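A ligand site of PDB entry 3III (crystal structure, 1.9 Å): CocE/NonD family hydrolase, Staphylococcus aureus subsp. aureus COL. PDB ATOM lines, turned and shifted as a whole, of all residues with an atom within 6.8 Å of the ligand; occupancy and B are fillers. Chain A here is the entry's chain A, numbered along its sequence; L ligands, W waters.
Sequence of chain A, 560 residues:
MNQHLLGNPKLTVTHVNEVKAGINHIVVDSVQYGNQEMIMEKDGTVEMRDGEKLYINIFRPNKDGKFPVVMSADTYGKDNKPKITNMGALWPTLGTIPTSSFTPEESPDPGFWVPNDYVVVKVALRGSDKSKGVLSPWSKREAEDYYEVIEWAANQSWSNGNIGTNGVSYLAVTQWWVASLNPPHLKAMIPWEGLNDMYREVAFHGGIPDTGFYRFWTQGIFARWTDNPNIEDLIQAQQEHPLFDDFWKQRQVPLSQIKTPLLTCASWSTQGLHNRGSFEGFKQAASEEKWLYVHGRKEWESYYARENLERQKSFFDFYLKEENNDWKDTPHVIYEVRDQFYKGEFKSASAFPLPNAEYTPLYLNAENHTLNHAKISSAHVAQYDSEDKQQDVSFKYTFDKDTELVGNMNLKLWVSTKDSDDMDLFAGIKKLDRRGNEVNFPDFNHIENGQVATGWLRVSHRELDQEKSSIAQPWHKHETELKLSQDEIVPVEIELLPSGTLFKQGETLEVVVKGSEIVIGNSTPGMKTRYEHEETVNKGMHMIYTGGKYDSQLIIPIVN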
ATOM      1  N   TYR A  76     -18.990  -5.822  17.178  1.00  0.00           N
ATOM      2  CA  TYR A  76     -20.432  -5.865  17.446  1.00  0.00           C
ATOM      3  C   TYR A  76     -21.074  -4.534  17.821  1.00  0.00           C
ATOM      4  O   TYR A  76     -22.292  -4.444  17.821  1.00  0.00           O
ATOM      5  CB  TYR A  76     -20.695  -6.872  18.560  1.00  0.00           C
ATOM      6  CG  TYR A  76     -20.373  -8.299  18.273  1.00  0.00           C
ATOM      7  CD1 TYR A  76     -20.266  -8.792  16.974  1.00  0.00           C
ATOM      8  CD2 TYR A  76     -20.307  -9.220  19.304  1.00  0.00           C
ATOM      9  CE1 TYR A  76     -20.031 -10.169  16.767  1.00  0.00           C
ATOM     10  CE2 TYR A  76     -20.105 -10.597  19.068  1.00  0.00           C
ATOM     11  CZ  TYR A  76     -19.977 -11.050  17.823  1.00  0.00           C
ATOM     12  OH  TYR A  76     -19.774 -12.434  17.614  1.00  0.00           O
ATOM     13  N   LYS A  83     -29.392  -6.042  25.792  1.00  0.00           N
ATOM     14  CA  LYS A  83     -30.826  -6.262  25.612  1.00  0.00           C
ATOM     15  C   LYS A  83     -31.453  -6.882  26.860  1.00  0.00           C
ATOM     16  O   LYS A  83     -31.046  -7.952  27.286  1.00  0.00           O
ATOM     17  CB  LYS A  83     -31.068  -7.156  24.417  1.00  0.00           C
ATOM     18  CG  LYS A  83     -30.722  -6.490  23.111  1.00  0.00           C
ATOM     19  CD  LYS A  83     -31.619  -7.000  21.987  1.00  0.00           C
ATOM     20  CE  LYS A  83     -30.965  -8.076  21.159  1.00  0.00           C
ATOM     21  NZ  LYS A  83     -31.875  -8.511  20.077  1.00  0.00           N
ATOM     22  N   MET A  87     -35.952 -10.424  26.259  1.00  0.00           N
ATOM     23  CA  MET A  87     -35.079 -11.593  26.135  1.00  0.00           C
ATOM     24  C   MET A  87     -35.553 -12.800  26.959  1.00  0.00           C
ATOM     25  O   MET A  87     -35.344 -13.948  26.577  1.00  0.00           O
ATOM     26  CB  MET A  87     -33.643 -11.225  26.522  1.00  0.00           C
ATOM     27  CG  MET A  87     -32.575 -11.979  25.751  1.00  0.00           C
ATOM     28  SD  MET A  87     -32.752 -11.885  23.768  1.00  0.00           S
ATOM     29  CE  MET A  87     -33.277  -9.990  23.565  1.00  0.00           C
ATOM     30  N   TRP A  91     -35.411 -15.696  24.362  1.00  0.00           N
ATOM     31  CA  TRP A  91     -34.294 -16.639  24.484  1.00  0.00           C
ATOM     32  C   TRP A  91     -34.214 -17.021  25.985  1.00  0.00           C
ATOM     33  O   TRP A  91     -33.375 -16.517  26.691  1.00  0.00           O
ATOM     34  CB  TRP A  91     -32.983 -16.054  23.987  1.00  0.00           C
ATOM     35  CG  TRP A  91     -31.918 -17.132  23.694  1.00  0.00           C
ATOM     36  CD1 TRP A  91     -32.047 -18.481  23.944  1.00  0.00           C
ATOM     37  CD2 TRP A  91     -30.618 -16.974  23.071  1.00  0.00           C
ATOM     38  NE1 TRP A  91     -30.918 -19.146  23.532  1.00  0.00           N
ATOM     39  CE2 TRP A  91     -30.025 -18.247  23.032  1.00  0.00           C
ATOM     40  CE3 TRP A  91     -29.890 -15.881  22.594  1.00  0.00           C
ATOM     41  CZ2 TRP A  91     -28.767 -18.466  22.457  1.00  0.00           C
ATOM     42  CZ3 TRP A  91     -28.628 -16.093  22.050  1.00  0.00           C
ATOM     43  CH2 TRP A  91     -28.079 -17.374  21.989  1.00  0.00           C
ATOM     44  N   LEU A  94     -30.968 -18.407  28.226  1.00  0.00           N
ATOM     45  CA  LEU A  94     -29.722 -17.628  28.363  1.00  0.00           C
ATOM     46  C   LEU A  94     -29.169 -17.551  29.773  1.00  0.00           C
ATOM     47  O   LEU A  94     -27.969 -17.272  29.949  1.00  0.00           O
ATOM     48  CB  LEU A  94     -29.870 -16.200  27.838  1.00  0.00           C
ATOM     49  CG  LEU A  94     -29.631 -16.017  26.348  1.00  0.00           C
ATOM     50  CD1 LEU A  94     -29.954 -14.555  26.009  1.00  0.00           C
ATOM     51  CD2 LEU A  94     -28.191 -16.412  25.959  1.00  0.00           C
ATOM     52  N   TRP A 138     -11.575 -12.103  13.094  1.00  0.00           N
ATOM     53  CA  TRP A 138     -10.770 -13.241  13.571  1.00  0.00           C
ATOM     54  C   TRP A 138      -9.649 -13.510  12.582  1.00  0.00           C
ATOM     55  O   TRP A 138      -9.434 -14.646  12.124  1.00  0.00           O
ATOM     56  CB  TRP A 138     -11.689 -14.455  13.835  1.00  0.00           C
ATOM     57  CG  TRP A 138     -12.752 -14.202  14.811  1.00  0.00           C
ATOM     58  CD1 TRP A 138     -12.803 -13.143  15.694  1.00  0.00           C
ATOM     59  CD2 TRP A 138     -13.941 -14.979  15.083  1.00  0.00           C
ATOM     60  NE1 TRP A 138     -13.915 -13.222  16.460  1.00  0.00           N
ATOM     61  CE2 TRP A 138     -14.629 -14.343  16.111  1.00  0.00           C
ATOM     62  CE3 TRP A 138     -14.474 -16.162  14.562  1.00  0.00           C
ATOM     63  CZ2 TRP A 138     -15.837 -14.832  16.640  1.00  0.00           C
ATOM     64  CZ3 TRP A 138     -15.685 -16.672  15.115  1.00  0.00           C
ATOM     65  CH2 TRP A 138     -16.346 -15.997  16.116  1.00  0.00           C
ATOM     66  N   VAL A 168     -15.782 -12.328  26.380  1.00  0.00           N
ATOM     67  CA  VAL A 168     -16.414 -13.596  26.007  1.00  0.00           C
ATOM     68  C   VAL A 168     -16.629 -13.640  24.507  1.00  0.00           C
ATOM     69  O   VAL A 168     -16.932 -12.601  23.882  1.00  0.00           O
ATOM     70  CB  VAL A 168     -17.804 -13.724  26.734  1.00  0.00           C
ATOM     71  CG1 VAL A 168     -18.510 -15.008  26.371  1.00  0.00           C
ATOM     72  CG2 VAL A 168     -17.544 -13.632  28.304  1.00  0.00           C
ATOM     73  N   SER A 169     -16.504 -14.847  23.965  1.00  0.00           N
ATOM     74  CA  SER A 169     -16.889 -15.215  22.587  1.00  0.00           C
ATOM     75  C   SER A 169     -16.000 -14.396  21.622  1.00  0.00           C
ATOM     76  O   SER A 169     -14.792 -14.545  21.657  1.00  0.00           O
ATOM     77  CB  SER A 169     -18.383 -15.011  22.372  1.00  0.00           C
ATOM     78  OG  SER A 169     -18.736 -15.448  21.064  1.00  0.00           O
ATOM     79  N   TYR A 170     -16.550 -13.547  20.753  1.00  0.00           N
ATOM     80  CA  TYR A 170     -15.705 -12.745  19.805  1.00  0.00           C
ATOM     81  C   TYR A 170     -14.607 -11.997  20.616  1.00  0.00           C
ATOM     82  O   TYR A 170     -13.452 -11.914  20.201  1.00  0.00           O
ATOM     83  CB  TYR A 170     -16.550 -11.724  19.064  1.00  0.00           C
ATOM     84  CG  TYR A 170     -15.983 -11.101  17.824  1.00  0.00           C
ATOM     85  CD1 TYR A 170     -16.617 -11.282  16.593  1.00  0.00           C
ATOM     86  CD2 TYR A 170     -14.881 -10.243  17.860  1.00  0.00           C
ATOM     87  CE1 TYR A 170     -16.141 -10.681  15.429  1.00  0.00           C
ATOM     88  CE2 TYR A 170     -14.373  -9.635  16.697  1.00  0.00           C
ATOM     89  CZ  TYR A 170     -15.018  -9.876  15.480  1.00  0.00           C
ATOM     90  OH  TYR A 170     -14.550  -9.260  14.320  1.00  0.00           O
ATOM     91  N   LEU A 171     -14.982 -11.483  21.798  1.00  0.00           N
ATOM     92  CA  LEU A 171     -14.088 -10.753  22.680  1.00  0.00           C
ATOM     93  C   LEU A 171     -12.957 -11.626  23.273  1.00  0.00           C
ATOM     94  O   LEU A 171     -11.979 -11.093  23.832  1.00  0.00           O
ATOM     95  CB  LEU A 171     -14.872 -10.008  23.767  1.00  0.00           C
ATOM     96  CG  LEU A 171     -15.923  -8.945  23.353  1.00  0.00           C
ATOM     97  CD1 LEU A 171     -17.114  -9.460  22.611  1.00  0.00           C
ATOM     98  CD2 LEU A 171     -16.353  -8.228  24.662  1.00  0.00           C
ATOM     99  N   PHE A 213     -25.577 -21.628  12.802  1.00  0.00           N
ATOM    100  CA  PHE A 213     -24.918 -20.549  13.536  1.00  0.00           C
ATOM    101  C   PHE A 213     -23.867 -19.734  12.742  1.00  0.00           C
ATOM    102  O   PHE A 213     -23.908 -18.499  12.728  1.00  0.00           O
ATOM    103  CB  PHE A 213     -24.277 -21.018  14.824  1.00  0.00           C
ATOM    104  CG  PHE A 213     -23.634 -19.914  15.557  1.00  0.00           C
ATOM    105  CD1 PHE A 213     -24.393 -19.037  16.320  1.00  0.00           C
ATOM    106  CD2 PHE A 213     -22.270 -19.701  15.451  1.00  0.00           C
ATOM    107  CE1 PHE A 213     -23.760 -17.967  16.993  1.00  0.00           C
ATOM    108  CE2 PHE A 213     -21.653 -18.659  16.132  1.00  0.00           C
ATOM    109  CZ  PHE A 213     -22.404 -17.794  16.899  1.00  0.00           C
ATOM    110  N   PHE A 216     -25.676 -17.514  10.410  1.00  0.00           N
ATOM    111  CA  PHE A 216     -26.435 -16.548  11.225  1.00  0.00           C
ATOM    112  C   PHE A 216     -25.505 -15.434  11.775  1.00  0.00           C
ATOM    113  O   PHE A 216     -25.798 -14.213  11.709  1.00  0.00           O
ATOM    114  CB  PHE A 216     -27.048 -17.320  12.361  1.00  0.00           C
ATOM    115  CG  PHE A 216     -27.594 -16.466  13.495  1.00  0.00           C
ATOM    116  CD1 PHE A 216     -28.798 -15.797  13.346  1.00  0.00           C
ATOM    117  CD2 PHE A 216     -26.934 -16.410  14.723  1.00  0.00           C
ATOM    118  CE1 PHE A 216     -29.307 -15.043  14.403  1.00  0.00           C
ATOM    119  CE2 PHE A 216     -27.461 -15.694  15.770  1.00  0.00           C
ATOM    120  CZ  PHE A 216     -28.644 -15.004  15.582  1.00  0.00           C
ATOM    121  N   TRP A 217     -24.347 -15.870  12.241  1.00  0.00           N
ATOM    122  CA  TRP A 217     -23.342 -15.006  12.827  1.00  0.00           C
ATOM    123  C   TRP A 217     -22.798 -14.083  11.746  1.00  0.00           C
ATOM    124  O   TRP A 217     -22.696 -12.856  11.932  1.00  0.00           O
ATOM    125  CB  TRP A 217     -22.255 -15.893  13.424  1.00  0.00           C
ATOM    126  CG  TRP A 217     -21.055 -15.176  13.839  1.00  0.00           C
ATOM    127  CD1 TRP A 217     -20.914 -14.399  14.931  1.00  0.00           C
ATOM    128  CD2 TRP A 217     -19.787 -15.162  13.164  1.00  0.00           C
ATOM    129  NE1 TRP A 217     -19.644 -13.875  14.965  1.00  0.00           N
ATOM    130  CE2 TRP A 217     -18.933 -14.335  13.903  1.00  0.00           C
ATOM    131  CE3 TRP A 217     -19.295 -15.765  12.000  1.00  0.00           C
ATOM    132  CZ2 TRP A 217     -17.605 -14.113  13.529  1.00  0.00           C
ATOM    133  CZ3 TRP A 217     -17.956 -15.544  11.648  1.00  0.00           C
ATOM    134  CH2 TRP A 217     -17.143 -14.715  12.381  1.00  0.00           C
ATOM    135  N   LEU A 273     -18.906 -24.655  19.138  1.00  0.00           N
ATOM    136  CA  LEU A 273     -18.423 -23.285  18.919  1.00  0.00           C
ATOM    137  C   LEU A 273     -17.095 -23.110  19.681  1.00  0.00           C
ATOM    138  O   LEU A 273     -16.054 -23.462  19.139  1.00  0.00           O
ATOM    139  CB  LEU A 273     -19.470 -22.253  19.316  1.00  0.00           C
ATOM    140  CG  LEU A 273     -19.117 -20.805  18.900  1.00  0.00           C
ATOM    141  CD1 LEU A 273     -18.933 -20.682  17.373  1.00  0.00           C
ATOM    142  CD2 LEU A 273     -20.212 -19.845  19.417  1.00  0.00           C
ATOM    143  N   HIS A 274     -17.106 -22.627  20.910  1.00  0.00           N
ATOM    144  CA  HIS A 274     -15.846 -22.258  21.584  1.00  0.00           C
ATOM    145  C   HIS A 274     -15.064 -23.340  22.324  1.00  0.00           C
ATOM    146  O   HIS A 274     -13.897 -23.128  22.673  1.00  0.00           O
ATOM    147  CB  HIS A 274     -16.059 -21.046  22.500  1.00  0.00           C
ATOM    148  CG  HIS A 274     -16.631 -19.851  21.810  1.00  0.00           C
ATOM    149  ND1 HIS A 274     -16.028 -19.246  20.725  1.00  0.00           N
ATOM    150  CD2 HIS A 274     -17.781 -19.177  22.034  1.00  0.00           C
ATOM    151  CE1 HIS A 274     -16.766 -18.213  20.345  1.00  0.00           C
ATOM    152  NE2 HIS A 274     -17.839 -18.153  21.118  1.00  0.00           N
ATOM    153  N   GLU A 299     -22.945 -19.745  29.433  1.00  0.00           N
ATOM    154  CA  GLU A 299     -21.765 -18.965  29.009  1.00  0.00           C
ATOM    155  C   GLU A 299     -21.617 -17.590  29.628  1.00  0.00           C
ATOM    156  O   GLU A 299     -20.685 -17.375  30.449  1.00  0.00           O
ATOM    157  CB  GLU A 299     -21.745 -18.893  27.471  1.00  0.00           C
ATOM    158  CG  GLU A 299     -20.661 -18.054  26.786  1.00  0.00           C
ATOM    159  CD  GLU A 299     -20.860 -18.011  25.280  1.00  0.00           C
ATOM    160  OE1 GLU A 299     -21.706 -18.775  24.783  1.00  0.00           O
ATOM    161  OE2 GLU A 299     -20.226 -17.215  24.559  1.00  0.00           O
ATOM    162  N   TRP A 300     -22.490 -16.672  29.256  1.00  0.00           N
ATOM    163  CA  TRP A 300     -22.430 -15.297  29.773  1.00  0.00           C
ATOM    164  C   TRP A 300     -22.846 -15.292  31.255  1.00  0.00           C
ATOM    165  O   TRP A 300     -22.315 -14.516  32.058  1.00  0.00           O
ATOM    166  CB  TRP A 300     -23.309 -14.329  28.976  1.00  0.00           C
ATOM    167  CG  TRP A 300     -22.818 -14.138  27.566  1.00  0.00           C
ATOM    168  CD1 TRP A 300     -21.786 -13.333  27.143  1.00  0.00           C
ATOM    169  CD2 TRP A 300     -23.325 -14.777  26.389  1.00  0.00           C
ATOM    170  NE1 TRP A 300     -21.619 -13.450  25.781  1.00  0.00           N
ATOM    171  CE2 TRP A 300     -22.532 -14.346  25.302  1.00  0.00           C
ATOM    172  CE3 TRP A 300     -24.361 -15.704  26.160  1.00  0.00           C
ATOM    173  CZ2 TRP A 300     -22.764 -14.743  23.995  1.00  0.00           C
ATOM    174  CZ3 TRP A 300     -24.587 -16.132  24.882  1.00  0.00           C
ATOM    175  CH2 TRP A 300     -23.777 -15.667  23.795  1.00  0.00           C
ATOM    176  N   ASN A 445     -26.775 -24.261  21.410  1.00  0.00           N
ATOM    177  CA  ASN A 445     -26.346 -22.996  21.961  1.00  0.00           C
ATOM    178  C   ASN A 445     -27.382 -22.636  23.045  1.00  0.00           C
ATOM    179  O   ASN A 445     -28.551 -22.254  22.741  1.00  0.00           O
ATOM    180  CB  ASN A 445     -26.245 -21.962  20.789  1.00  0.00           C
ATOM    181  CG  ASN A 445     -25.747 -20.611  21.208  1.00  0.00           C
ATOM    182  OD1 ASN A 445     -25.575 -20.388  22.426  1.00  0.00           O
ATOM    183  ND2 ASN A 445     -25.568 -19.667  20.261  1.00  0.00           N
ATOM    184  N   THR A 524     -34.151 -21.164  20.222  1.00  0.00           N
ATOM    185  CA  THR A 524     -34.677 -19.927  19.651  1.00  0.00           C
ATOM    186  C   THR A 524     -35.394 -20.287  18.316  1.00  0.00           C
ATOM    187  O   THR A 524     -34.847 -20.022  17.239  1.00  0.00           O
ATOM    188  CB  THR A 524     -33.556 -18.873  19.372  1.00  0.00           C
ATOM    189  OG1 THR A 524     -32.597 -19.412  18.439  1.00  0.00           O
ATOM    190  CG2 THR A 524     -32.785 -18.532  20.650  1.00  0.00           C
ATOM    191  N   MET A 527     -34.752 -18.804  14.573  1.00  0.00           N
ATOM    192  CA  MET A 527     -33.476 -18.130  14.545  1.00  0.00           C
ATOM    193  C   MET A 527     -32.363 -19.121  14.742  1.00  0.00           C
ATOM    194  O   MET A 527     -32.403 -19.925  15.666  1.00  0.00           O
ATOM    195  CB  MET A 527     -33.415 -17.091  15.640  1.00  0.00           C
ATOM    196  CG  MET A 527     -32.174 -16.290  15.638  1.00  0.00           C
ATOM    197  SD  MET A 527     -32.296 -14.923  17.032  1.00  0.00           S
ATOM    198  CE  MET A 527     -33.742 -13.869  16.204  1.00  0.00           C
ATOM    199  N   THR A 529     -29.490 -19.931  16.042  1.00  0.00           N
ATOM    200  CA  THR A 529     -28.448 -19.736  17.052  1.00  0.00           C
ATOM    201  C   THR A 529     -27.577 -20.974  17.283  1.00  0.00           C
ATOM    202  O   THR A 529     -26.470 -20.858  17.791  1.00  0.00           O
ATOM    203  CB  THR A 529     -29.035 -19.317  18.432  1.00  0.00           C
ATOM    204  OG1 THR A 529     -29.932 -20.313  18.848  1.00  0.00           O
ATOM    205  CG2 THR A 529     -29.744 -17.971  18.344  1.00  0.00           C
HETATM  206  C1  LIG L   1     -21.568 -14.407  19.846  1.00  0.00           C
HETATM  207  O1  LIG L   1     -20.408 -14.022  19.700  1.00  0.00           O
HETATM  208  O2  LIG L   1     -21.778 -15.353  20.625  1.00  0.00           O
HETATM  209  C2  LIG L   1     -22.651 -13.746  19.051  1.00  0.00           C
HETATM  210  C3  LIG L   1     -24.041 -14.155  19.508  1.00  0.00           C
HETATM  211  C4  LIG L   1     -25.200 -13.400  18.848  1.00  0.00           C
HETATM  212  C5  LIG L   1     -26.569 -13.622  19.543  1.00  0.00           C
HETATM  213  C6  LIG L   1     -27.835 -13.443  18.661  1.00  0.00           C
HETATM  214  C7  LIG L   1     -28.992 -12.526  19.132  1.00  0.00           C
HETATM  215  C8  LIG L   1     -30.218 -13.205  19.809  1.00  0.00           C
HETATM  216  O   HOH W   1     -23.991 -17.252  20.835  1.00  0.00           O
HETATM  217  O   HOH W   2     -20.713 -17.430  22.039  1.00  0.00           O
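The side-chain hydroxyl (OH) of Tyr 76 lies within hydrogen-bond range of an oxygen (O1) of the ligand (2.7 Å). An oxygen (O1) of the ligand is in hydrogen-bond range of the side-chain hydroxyl (OG) of Ser 169 (2.6 Å).
The backbone carbonyl oxygen of Met 527 lies within hydrogen-bond range of the side-chain hydroxyl of Thr 524 (2.8 Å). A ring nitrogen (NE2) of His 274 sits at hydrogen-bond distance from the side-chain hydroxyl (OG) of Ser 169, at 2.9 Å. The indole nitrogen (NE1) of Trp 217 lies within hydrogen-bond range of the side-chain hydroxyl (OH) of Tyr 76, at 3.0 Å.
Merely in contact with the ligand: Phe 216 (3.5 Å), Trp 300 (3.6 Å), Met 527 (3.9 Å) and Trp 91 (3.9 Å). Hydrophobic or aromatic side chains within 4 Å of the ligand: Tyr 76, Trp 91, Phe 216, Trp 300 and Met 527. Of the 21 residues printed, 6 come within 4 Å of the ligand. Along chain A the residues within 4 Å of the ligand span positions 76 to 527. The nearest printed residue that does not touch the ligand is Tyr 170 (4.03 Å).
Water W2 lies within hydrogen-bond range of OE2 of Glu 299 (2.6 Å), O2 of the ligand (2.7 Å), OG of Ser 169 (3.0 Å) and NE2 of His 274 (3.1 Å). Water W1 bridges O2 of the ligand (2.9 Å) and ND2 of Asn 445 (2.9 Å).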
